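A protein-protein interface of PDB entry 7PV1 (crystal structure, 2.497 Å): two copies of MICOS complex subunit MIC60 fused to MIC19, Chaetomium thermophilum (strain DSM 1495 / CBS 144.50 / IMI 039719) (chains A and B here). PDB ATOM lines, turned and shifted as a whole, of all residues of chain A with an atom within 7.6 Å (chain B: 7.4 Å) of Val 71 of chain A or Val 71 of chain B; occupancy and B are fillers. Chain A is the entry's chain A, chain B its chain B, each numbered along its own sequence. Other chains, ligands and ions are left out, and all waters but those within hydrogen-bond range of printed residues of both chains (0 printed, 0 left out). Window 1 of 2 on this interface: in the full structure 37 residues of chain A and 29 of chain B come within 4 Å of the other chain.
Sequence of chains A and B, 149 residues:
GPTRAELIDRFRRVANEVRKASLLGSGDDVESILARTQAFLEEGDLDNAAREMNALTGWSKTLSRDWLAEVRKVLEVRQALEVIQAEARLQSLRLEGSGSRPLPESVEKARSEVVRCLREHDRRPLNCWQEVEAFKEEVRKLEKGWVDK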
ATOM      1  N   LEU A  23      -8.342   1.301   3.622  1.00  0.00           N
ATOM      2  CA  LEU A  23      -8.170   2.403   4.565  1.00  0.00           C
ATOM      3  C   LEU A  23      -8.509   1.965   5.983  1.00  0.00           C
ATOM      4  O   LEU A  23      -7.842   2.371   6.942  1.00  0.00           O
ATOM      5  CB  LEU A  23      -9.036   3.597   4.157  1.00  0.00           C
ATOM      6  CG  LEU A  23      -8.442   4.628   3.196  1.00  0.00           C
ATOM      7  CD1 LEU A  23      -9.411   5.783   2.981  1.00  0.00           C
ATOM      8  CD2 LEU A  23      -7.114   5.144   3.728  1.00  0.00           C
ATOM      9  N   ARG A  65      -8.533   7.668  13.513  1.00  0.00           N
ATOM     10  CA  ARG A  65      -7.533   8.718  13.389  1.00  0.00           C
ATOM     11  C   ARG A  65      -6.555   8.400  12.268  1.00  0.00           C
ATOM     12  O   ARG A  65      -6.068   9.311  11.588  1.00  0.00           O
ATOM     13  CB  ARG A  65      -6.793   8.895  14.715  1.00  0.00           C
ATOM     14  N   ASP A  66      -6.257   7.114  12.070  1.00  0.00           N
ATOM     15  CA  ASP A  66      -5.282   6.706  11.065  1.00  0.00           C
ATOM     16  C   ASP A  66      -5.730   7.087   9.657  1.00  0.00           C
ATOM     17  O   ASP A  66      -4.990   7.745   8.916  1.00  0.00           O
ATOM     18  CB  ASP A  66      -5.064   5.194  11.164  1.00  0.00           C
ATOM     19  CG  ASP A  66      -3.996   4.692  10.214  1.00  0.00           C
ATOM     20  OD1 ASP A  66      -3.295   5.528   9.606  1.00  0.00           O
ATOM     21  OD2 ASP A  66      -3.856   3.459  10.074  1.00  0.00           O
ATOM     22  N   TRP A  67      -6.935   6.666   9.264  1.00  0.00           N
ATOM     23  CA  TRP A  67      -7.412   6.903   7.904  1.00  0.00           C
ATOM     24  C   TRP A  67      -7.922   8.326   7.673  1.00  0.00           C
ATOM     25  O   TRP A  67      -7.804   8.835   6.553  1.00  0.00           O
ATOM     26  CB  TRP A  67      -8.480   5.866   7.539  1.00  0.00           C
ATOM     27  CG  TRP A  67      -9.802   6.019   8.222  1.00  0.00           C
ATOM     28  CD1 TRP A  67     -10.235   5.354   9.334  1.00  0.00           C
ATOM     29  CD2 TRP A  67     -10.886   6.857   7.809  1.00  0.00           C
ATOM     30  NE1 TRP A  67     -11.514   5.745   9.650  1.00  0.00           N
ATOM     31  CE2 TRP A  67     -11.936   6.665   8.728  1.00  0.00           C
ATOM     32  CE3 TRP A  67     -11.066   7.758   6.756  1.00  0.00           C
ATOM     33  CZ2 TRP A  67     -13.148   7.343   8.626  1.00  0.00           C
ATOM     34  CZ3 TRP A  67     -12.267   8.427   6.658  1.00  0.00           C
ATOM     35  CH2 TRP A  67     -13.294   8.217   7.585  1.00  0.00           C
ATOM     36  N   LEU A  68      -8.488   8.985   8.689  1.00  0.00           N
ATOM     37  CA  LEU A  68      -8.899  10.377   8.503  1.00  0.00           C
ATOM     38  C   LEU A  68      -7.716  11.268   8.140  1.00  0.00           C
ATOM     39  O   LEU A  68      -7.842  12.163   7.296  1.00  0.00           O
ATOM     40  CB  LEU A  68      -9.616  10.914   9.745  1.00  0.00           C
ATOM     41  CG  LEU A  68     -11.126  10.666   9.829  1.00  0.00           C
ATOM     42  CD1 LEU A  68     -11.665  10.919  11.233  1.00  0.00           C
ATOM     43  CD2 LEU A  68     -11.846  11.551   8.814  1.00  0.00           C
ATOM     44  N   ALA A  69      -6.555  11.043   8.760  1.00  0.00           N
ATOM     45  CA  ALA A  69      -5.389  11.845   8.408  1.00  0.00           C
ATOM     46  C   ALA A  69      -5.041  11.683   6.936  1.00  0.00           C
ATOM     47  O   ALA A  69      -4.624  12.644   6.277  1.00  0.00           O
ATOM     48  CB  ALA A  69      -4.197  11.464   9.287  1.00  0.00           C
ATOM     49  N   GLU A  70      -5.214  10.475   6.395  1.00  0.00           N
ATOM     50  CA  GLU A  70      -4.901  10.242   4.989  1.00  0.00           C
ATOM     51  C   GLU A  70      -5.834  11.033   4.081  1.00  0.00           C
ATOM     52  O   GLU A  70      -5.384  11.692   3.136  1.00  0.00           O
ATOM     53  CB  GLU A  70      -4.974   8.747   4.675  1.00  0.00           C
ATOM     54  CG  GLU A  70      -3.825   7.943   5.258  1.00  0.00           C
ATOM     55  CD  GLU A  70      -3.815   6.506   4.779  1.00  0.00           C
ATOM     56  OE1 GLU A  70      -4.305   5.624   5.516  1.00  0.00           O
ATOM     57  OE2 GLU A  70      -3.320   6.258   3.659  1.00  0.00           O
ATOM     58  N   VAL A  71      -7.140  10.979   4.351  1.00  0.00           N
ATOM     59  CA  VAL A  71      -8.093  11.750   3.555  1.00  0.00           C
ATOM     60  C   VAL A  71      -7.793  13.240   3.662  1.00  0.00           C
ATOM     61  O   VAL A  71      -7.935  13.989   2.688  1.00  0.00           O
ATOM     62  CB  VAL A  71      -9.537  11.433   3.989  1.00  0.00           C
ATOM     63  CG1 VAL A  71     -10.523  12.325   3.254  1.00  0.00           C
ATOM     64  CG2 VAL A  71      -9.858   9.964   3.748  1.00  0.00           C
ATOM     65  N   ARG A  72      -7.360  13.693   4.841  1.00  0.00           N
ATOM     66  CA  ARG A  72      -7.127  15.121   5.032  1.00  0.00           C
ATOM     67  C   ARG A  72      -5.924  15.603   4.230  1.00  0.00           C
ATOM     68  O   ARG A  72      -5.971  16.679   3.621  1.00  0.00           O
ATOM     69  CB  ARG A  72      -6.944  15.438   6.517  1.00  0.00           C
ATOM     70  CG  ARG A  72      -6.430  16.847   6.772  1.00  0.00           C
ATOM     71  CD  ARG A  72      -6.648  17.301   8.206  1.00  0.00           C
ATOM     72  NE  ARG A  72      -6.232  16.303   9.188  1.00  0.00           N
ATOM     73  CZ  ARG A  72      -7.042  15.763  10.093  1.00  0.00           C
ATOM     74  NH1 ARG A  72      -8.316  16.134  10.155  1.00  0.00           N
ATOM     75  NH2 ARG A  72      -6.579  14.859  10.946  1.00  0.00           N
ATOM     76  N   LYS A  73      -4.839  14.827   4.211  1.00  0.00           N
ATOM     77  CA  LYS A  73      -3.647  15.267   3.498  1.00  0.00           C
ATOM     78  C   LYS A  73      -3.797  15.144   1.988  1.00  0.00           C
ATOM     79  O   LYS A  73      -3.197  15.929   1.246  1.00  0.00           O
ATOM     80  CB  LYS A  73      -2.420  14.491   3.977  1.00  0.00           C
ATOM     81  CG  LYS A  73      -1.467  15.343   4.808  1.00  0.00           C
ATOM     82  CD  LYS A  73      -0.189  14.608   5.173  1.00  0.00           C
ATOM     83  CE  LYS A  73       0.897  15.591   5.591  1.00  0.00           C
ATOM     84  NZ  LYS A  73       1.349  16.435   4.446  1.00  0.00           N
ATOM     85  N   VAL A  74      -4.578  14.174   1.509  1.00  0.00           N
ATOM     86  CA  VAL A  74      -4.871  14.129   0.081  1.00  0.00           C
ATOM     87  C   VAL A  74      -5.568  15.417  -0.335  1.00  0.00           C
ATOM     88  O   VAL A  74      -5.272  15.999  -1.387  1.00  0.00           O
ATOM     89  CB  VAL A  74      -5.712  12.882  -0.253  1.00  0.00           C
ATOM     90  CG1 VAL A  74      -6.744  13.195  -1.342  1.00  0.00           C
ATOM     91  CG2 VAL A  74      -4.805  11.697  -0.628  1.00  0.00           C
ATOM     92  N   LEU A  75      -6.497  15.888   0.500  1.00  0.00           N
ATOM     93  CA  LEU A  75      -7.187  17.146   0.245  1.00  0.00           C
ATOM     94  C   LEU A  75      -6.227  18.329   0.340  1.00  0.00           C
ATOM     95  O   LEU A  75      -6.306  19.267  -0.462  1.00  0.00           O
ATOM     96  CB  LEU A  75      -8.343  17.306   1.235  1.00  0.00           C
ATOM     97  CG  LEU A  75      -9.509  16.324   1.081  1.00  0.00           C
ATOM     98  CD1 LEU A  75     -10.569  16.531   2.167  1.00  0.00           C
ATOM     99  CD2 LEU A  75     -10.124  16.421  -0.304  1.00  0.00           C
ATOM    100  N   GLU A  76      -5.325  18.308   1.325  1.00  0.00           N
ATOM    101  CA  GLU A  76      -4.373  19.402   1.487  1.00  0.00           C
ATOM    102  C   GLU A  76      -3.458  19.512   0.275  1.00  0.00           C
ATOM    103  O   GLU A  76      -3.284  20.597  -0.294  1.00  0.00           O
ATOM    104  CB  GLU A  76      -3.545  19.176   2.752  1.00  0.00           C
ATOM    105  CG  GLU A  76      -4.270  19.430   4.057  1.00  0.00           C
ATOM    106  CD  GLU A  76      -3.411  19.087   5.257  1.00  0.00           C
ATOM    107  OE1 GLU A  76      -2.248  18.677   5.053  1.00  0.00           O
ATOM    108  OE2 GLU A  76      -3.899  19.207   6.400  1.00  0.00           O
ATOM    109  N   VAL A  77      -2.870  18.389  -0.141  1.00  0.00           N
ATOM    110  CA  VAL A  77      -1.988  18.392  -1.304  1.00  0.00           C
ATOM    111  C   VAL A  77      -2.764  18.770  -2.559  1.00  0.00           C
ATOM    112  O   VAL A  77      -2.263  19.497  -3.426  1.00  0.00           O
ATOM    113  CB  VAL A  77      -1.303  17.022  -1.454  1.00  0.00           C
ATOM    114  CG1 VAL A  77      -0.931  16.789  -2.896  1.00  0.00           C
ATOM    115  CG2 VAL A  77      -0.070  16.946  -0.573  1.00  0.00           C
ATOM    116  N   LEU A 126      -6.460  23.550   4.870  1.00  0.00           N
ATOM    117  CA  LEU A 126      -7.831  23.528   4.369  1.00  0.00           C
ATOM    118  C   LEU A 126      -8.665  24.699   4.878  1.00  0.00           C
ATOM    119  O   LEU A 126      -9.734  24.969   4.321  1.00  0.00           O
ATOM    120  CB  LEU A 126      -8.509  22.203   4.736  1.00  0.00           C
ATOM    121  CG  LEU A 126      -7.913  20.970   4.046  1.00  0.00           C
ATOM    122  CD1 LEU A 126      -8.651  19.692   4.427  1.00  0.00           C
ATOM    123  CD2 LEU A 126      -7.900  21.164   2.535  1.00  0.00           C
ATOM    124  N   LEU B  23      -2.636   7.997  -0.332  1.00  0.00           N
ATOM    125  CA  LEU B  23      -3.954   7.866  -0.951  1.00  0.00           C
ATOM    126  C   LEU B  23      -3.998   8.455  -2.355  1.00  0.00           C
ATOM    127  O   LEU B  23      -4.760   7.974  -3.201  1.00  0.00           O
ATOM    128  CB  LEU B  23      -5.031   8.516  -0.080  1.00  0.00           C
ATOM    129  CG  LEU B  23      -5.691   7.626   0.976  1.00  0.00           C
ATOM    130  CD1 LEU B  23      -6.813   8.371   1.686  1.00  0.00           C
ATOM    131  CD2 LEU B  23      -6.215   6.346   0.338  1.00  0.00           C
ATOM    132  N   ARG B  65     -11.137   9.255  -8.631  1.00  0.00           N
ATOM    133  CA  ARG B  65     -12.119   8.200  -8.407  1.00  0.00           C
ATOM    134  C   ARG B  65     -11.564   7.076  -7.536  1.00  0.00           C
ATOM    135  O   ARG B  65     -12.307   6.486  -6.741  1.00  0.00           O
ATOM    136  CB  ARG B  65     -12.615   7.639  -9.743  1.00  0.00           C
ATOM    137  CG  ARG B  65     -13.406   8.639 -10.562  1.00  0.00           C
ATOM    138  CD  ARG B  65     -13.964   8.021 -11.833  1.00  0.00           C
ATOM    139  NE  ARG B  65     -14.713   8.996 -12.621  1.00  0.00           N
ATOM    140  CZ  ARG B  65     -16.017   9.223 -12.488  1.00  0.00           C
ATOM    141  NH1 ARG B  65     -16.726   8.542 -11.598  1.00  0.00           N
ATOM    142  NH2 ARG B  65     -16.612  10.132 -13.248  1.00  0.00           N
ATOM    143  N   ASP B  66     -10.271   6.765  -7.667  1.00  0.00           N
ATOM    144  CA  ASP B  66      -9.708   5.648  -6.920  1.00  0.00           C
ATOM    145  C   ASP B  66      -9.832   5.874  -5.418  1.00  0.00           C
ATOM    146  O   ASP B  66     -10.392   5.040  -4.697  1.00  0.00           O
ATOM    147  CB  ASP B  66      -8.241   5.448  -7.311  1.00  0.00           C
ATOM    148  CG  ASP B  66      -8.072   4.989  -8.747  1.00  0.00           C
ATOM    149  OD1 ASP B  66      -8.992   4.330  -9.273  1.00  0.00           O
ATOM    150  OD2 ASP B  66      -7.016   5.283  -9.347  1.00  0.00           O
ATOM    151  N   TRP B  67      -9.325   7.005  -4.928  1.00  0.00           N
ATOM    152  CA  TRP B  67      -9.375   7.279  -3.496  1.00  0.00           C
ATOM    153  C   TRP B  67     -10.760   7.718  -3.032  1.00  0.00           C
ATOM    154  O   TRP B  67     -11.123   7.462  -1.878  1.00  0.00           O
ATOM    155  CB  TRP B  67      -8.289   8.295  -3.116  1.00  0.00           C
ATOM    156  CG  TRP B  67      -8.480   9.695  -3.610  1.00  0.00           C
ATOM    157  CD1 TRP B  67      -7.916  10.250  -4.721  1.00  0.00           C
ATOM    158  CD2 TRP B  67      -9.248  10.735  -2.991  1.00  0.00           C
ATOM    159  NE1 TRP B  67      -8.301  11.562  -4.846  1.00  0.00           N
ATOM    160  CE2 TRP B  67      -9.119  11.884  -3.797  1.00  0.00           C
ATOM    161  CE3 TRP B  67     -10.043  10.803  -1.842  1.00  0.00           C
ATOM    162  CZ2 TRP B  67      -9.753  13.086  -3.491  1.00  0.00           C
ATOM    163  CZ3 TRP B  67     -10.669  11.997  -1.540  1.00  0.00           C
ATOM    164  CH2 TRP B  67     -10.521  13.122  -2.360  1.00  0.00           C
ATOM    165  N   LEU B  68     -11.545   8.373  -3.891  1.00  0.00           N
ATOM    166  CA  LEU B  68     -12.916   8.700  -3.506  1.00  0.00           C
ATOM    167  C   LEU B  68     -13.717   7.438  -3.212  1.00  0.00           C
ATOM    168  O   LEU B  68     -14.460   7.379  -2.225  1.00  0.00           O
ATOM    169  CB  LEU B  68     -13.593   9.523  -4.602  1.00  0.00           C
ATOM    170  CG  LEU B  68     -13.332  11.029  -4.596  1.00  0.00           C
ATOM    171  CD1 LEU B  68     -13.753  11.660  -5.918  1.00  0.00           C
ATOM    172  CD2 LEU B  68     -14.049  11.689  -3.432  1.00  0.00           C
ATOM    173  N   ALA B  69     -13.572   6.409  -4.049  1.00  0.00           N
ATOM    174  CA  ALA B  69     -14.237   5.142  -3.766  1.00  0.00           C
ATOM    175  C   ALA B  69     -13.712   4.537  -2.471  1.00  0.00           C
ATOM    176  O   ALA B  69     -14.480   3.988  -1.671  1.00  0.00           O
ATOM    177  CB  ALA B  69     -14.048   4.173  -4.934  1.00  0.00           C
ATOM    178  N   GLU B  70     -12.399   4.635  -2.248  1.00  0.00           N
ATOM    179  CA  GLU B  70     -11.813   4.138  -1.009  1.00  0.00           C
ATOM    180  C   GLU B  70     -12.428   4.824   0.203  1.00  0.00           C
ATOM    181  O   GLU B  70     -12.678   4.182   1.230  1.00  0.00           O
ATOM    182  CB  GLU B  70     -10.298   4.345  -1.027  1.00  0.00           C
ATOM    183  CG  GLU B  70      -9.552   3.548  -2.091  1.00  0.00           C
ATOM    184  CD  GLU B  70      -9.018   2.227  -1.568  1.00  0.00           C
ATOM    185  OE1 GLU B  70      -9.669   1.183  -1.791  1.00  0.00           O
ATOM    186  OE2 GLU B  70      -7.946   2.235  -0.927  1.00  0.00           O
ATOM    187  N   VAL B  71     -12.678   6.132   0.104  1.00  0.00           N
ATOM    188  CA  VAL B  71     -13.261   6.864   1.224  1.00  0.00           C
ATOM    189  C   VAL B  71     -14.730   6.502   1.386  1.00  0.00           C
ATOM    190  O   VAL B  71     -15.247   6.427   2.508  1.00  0.00           O
ATOM    191  CB  VAL B  71     -13.064   8.378   1.030  1.00  0.00           C
ATOM    192  CG1 VAL B  71     -13.763   9.154   2.134  1.00  0.00           C
ATOM    193  CG2 VAL B  71     -11.582   8.713   0.980  1.00  0.00           C
ATOM    194  N   ARG B  72     -15.424   6.267   0.272  1.00  0.00           N
ATOM    195  CA  ARG B  72     -16.822   5.859   0.338  1.00  0.00           C
ATOM    196  C   ARG B  72     -16.965   4.496   1.002  1.00  0.00           C
ATOM    197  O   ARG B  72     -17.822   4.306   1.874  1.00  0.00           O
ATOM    198  CB  ARG B  72     -17.433   5.832  -1.062  1.00  0.00           C
ATOM    199  CG  ARG B  72     -18.945   5.753  -1.052  1.00  0.00           C
ATOM    200  CD  ARG B  72     -19.492   5.157  -2.334  1.00  0.00           C
ATOM    201  NE  ARG B  72     -18.946   5.795  -3.529  1.00  0.00           N
ATOM    202  CZ  ARG B  72     -18.054   5.229  -4.338  1.00  0.00           C
ATOM    203  NH1 ARG B  72     -17.608   4.004  -4.085  1.00  0.00           N
ATOM    204  NH2 ARG B  72     -17.613   5.883  -5.405  1.00  0.00           N
ATOM    205  N   LYS B  73     -16.137   3.528   0.598  1.00  0.00           N
ATOM    206  CA  LYS B  73     -16.217   2.202   1.201  1.00  0.00           C
ATOM    207  C   LYS B  73     -16.000   2.268   2.706  1.00  0.00           C
ATOM    208  O   LYS B  73     -16.638   1.528   3.464  1.00  0.00           O
ATOM    209  CB  LYS B  73     -15.193   1.263   0.567  1.00  0.00           C
ATOM    210  CG  LYS B  73     -15.380   1.013  -0.917  1.00  0.00           C
ATOM    211  CD  LYS B  73     -14.262   0.116  -1.435  1.00  0.00           C
ATOM    212  CE  LYS B  73     -14.039   0.303  -2.924  1.00  0.00           C
ATOM    213  NZ  LYS B  73     -12.690  -0.182  -3.329  1.00  0.00           N
ATOM    214  N   VAL B  74     -15.101   3.144   3.160  1.00  0.00           N
ATOM    215  CA  VAL B  74     -14.796   3.212   4.585  1.00  0.00           C
ATOM    216  C   VAL B  74     -15.963   3.816   5.354  1.00  0.00           C
ATOM    217  O   VAL B  74     -16.341   3.326   6.425  1.00  0.00           O
ATOM    218  CB  VAL B  74     -13.499   4.006   4.820  1.00  0.00           C
ATOM    219  CG1 VAL B  74     -13.230   4.147   6.311  1.00  0.00           C
ATOM    220  CG2 VAL B  74     -12.330   3.336   4.123  1.00  0.00           C
ATOM    221  N   LEU B  75     -16.563   4.879   4.817  1.00  0.00           N
ATOM    222  CA  LEU B  75     -17.698   5.498   5.491  1.00  0.00           C
ATOM    223  C   LEU B  75     -18.891   4.554   5.529  1.00  0.00           C
ATOM    224  O   LEU B  75     -19.596   4.471   6.541  1.00  0.00           O
ATOM    225  CB  LEU B  75     -18.060   6.813   4.802  1.00  0.00           C
ATOM    226  CG  LEU B  75     -17.016   7.917   4.975  1.00  0.00           C
ATOM    227  CD1 LEU B  75     -17.412   9.152   4.199  1.00  0.00           C
ATOM    228  CD2 LEU B  75     -16.822   8.249   6.443  1.00  0.00           C
ATOM    229  N   GLU B  76     -19.139   3.840   4.430  1.00  0.00           N
ATOM    230  CA  GLU B  76     -20.255   2.903   4.396  1.00  0.00           C
ATOM    231  C   GLU B  76     -20.065   1.786   5.414  1.00  0.00           C
ATOM    232  O   GLU B  76     -20.997   1.440   6.151  1.00  0.00           O
ATOM    233  CB  GLU B  76     -20.417   2.324   2.990  1.00  0.00           C
ATOM    234  CG  GLU B  76     -21.024   3.289   1.985  1.00  0.00           C
ATOM    235  CD  GLU B  76     -21.109   2.700   0.588  1.00  0.00           C
ATOM    236  OE1 GLU B  76     -20.723   1.524   0.411  1.00  0.00           O
ATOM    237  OE2 GLU B  76     -21.550   3.416  -0.335  1.00  0.00           O
ATOM    238  N   VAL B  77     -18.862   1.208   5.472  1.00  0.00           N
ATOM    239  CA  VAL B  77     -18.606   0.116   6.407  1.00  0.00           C
ATOM    240  C   VAL B  77     -18.788   0.580   7.847  1.00  0.00           C
ATOM    241  O   VAL B  77     -19.320  -0.154   8.688  1.00  0.00           O
ATOM    242  CB  VAL B  77     -17.196  -0.458   6.174  1.00  0.00           C
ATOM    243  CG1 VAL B  77     -16.676  -1.110   7.443  1.00  0.00           C
ATOM    244  CG2 VAL B  77     -17.214  -1.452   5.031  1.00  0.00           C
ATOM    245  N   LEU B 126     -25.024   5.635   2.268  1.00  0.00           N
ATOM    246  CA  LEU B 126     -24.815   6.846   3.052  1.00  0.00           C
ATOM    247  C   LEU B 126     -26.026   7.770   3.025  1.00  0.00           C
ATOM    248  O   LEU B 126     -26.120   8.669   3.870  1.00  0.00           O
ATOM    249  CB  LEU B 126     -23.583   7.600   2.551  1.00  0.00           C
ATOM    250  CG  LEU B 126     -22.259   6.859   2.753  1.00  0.00           C
ATOM    251  CD1 LEU B 126     -21.082   7.700   2.267  1.00  0.00           C
ATOM    252  CD2 LEU B 126     -22.080   6.420   4.201  1.00  0.00           C
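Hydrophobic or aromatic side chains of chain A that line the printed part of chain B: Leu 23, Trp 67, Val 71, Val 74 and Leu 75.
Hydrophobic or aromatic side chains of chain B that line the printed part of chain A: Leu 23, Trp 67, Val 71, Val 74 and Leu 75.
Along chain B the printed residues that touch a printed residue of chain A span positions 23 to 75.
Among the printed residues, 10 pairs touch across the chains.
Among the printed residues, no Asp or Glu carboxylate lies within 4 Å of a Lys or Arg side-chain nitrogen of the other chain.
Leu 23 of chain A touches its own counterpart, Leu 23 of chain B.
Trp 67 of chain A touches Val 74 of chain B, and with the chains exchanged Val 74 of chain A touches Trp 67 of chain B.
Val 71 of chain A touches Leu 23 of chain B, but with the chains exchanged Leu 23 of chain A does not touch Val 71 of chain B (4.2 Å).
Val 71 of chain A touches its own counterpart, Val 71 of chain B.
Of the 10 pairs that touch across the chains among the printed residues, 8 have their exchanged pair printed and touching as well.
CD2 of Leu 23 of chain A touches CD2 of Leu 23 of chain B, at 3.7 Å.
Leu 23 of chain A touches Val 74 of chain B.
CG1 of Val 74 of chain B touches CE2 of Trp 67 of chain A (3.7 Å).
Trp 67 of chain A touches Leu 75 of chain B.
Leu 23 of chain B touches Glu 70 of chain A.
Val 71 of chain A touches Leu 23 of chain B (N to CD1, 3.7 Å).
Val 71 of chain B touches Val 71 of chain A (CG2 to CG2, 3.5 Å).
Val 74 of chain A touches Leu 23 of chain B (CG2 to CB, 3.2 Å).
Trp 67 of chain B touches Val 74 of chain A (CE2 to CG1, 3.7 Å).
CD2 of Leu 75 of chain A touches CH2 of Trp 67 of chain B, at 3.9 Å.
Printed residues of chain B within 4 Å of Glu 70 of chain A: Leu 23.
Of the printed residues of chain B, Val 74 of chain A touches Leu 23 and Trp 67.
Val 71 of chain B touches just one residue of chain A: Val 71 (3.5 Å).
Of the printed residues of chain A, Val 74 of chain B touches Leu 23 (3.3 Å) and Trp 67 (3.7 Å).
The nearest residue of chain A that does not touch Val 71 of chain B is Leu 23 of chain A (4.2 Å).
The nearest printed residue of chain A that does not touch Trp 67 of chain B is Val 71 of chain A (4.8 Å).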
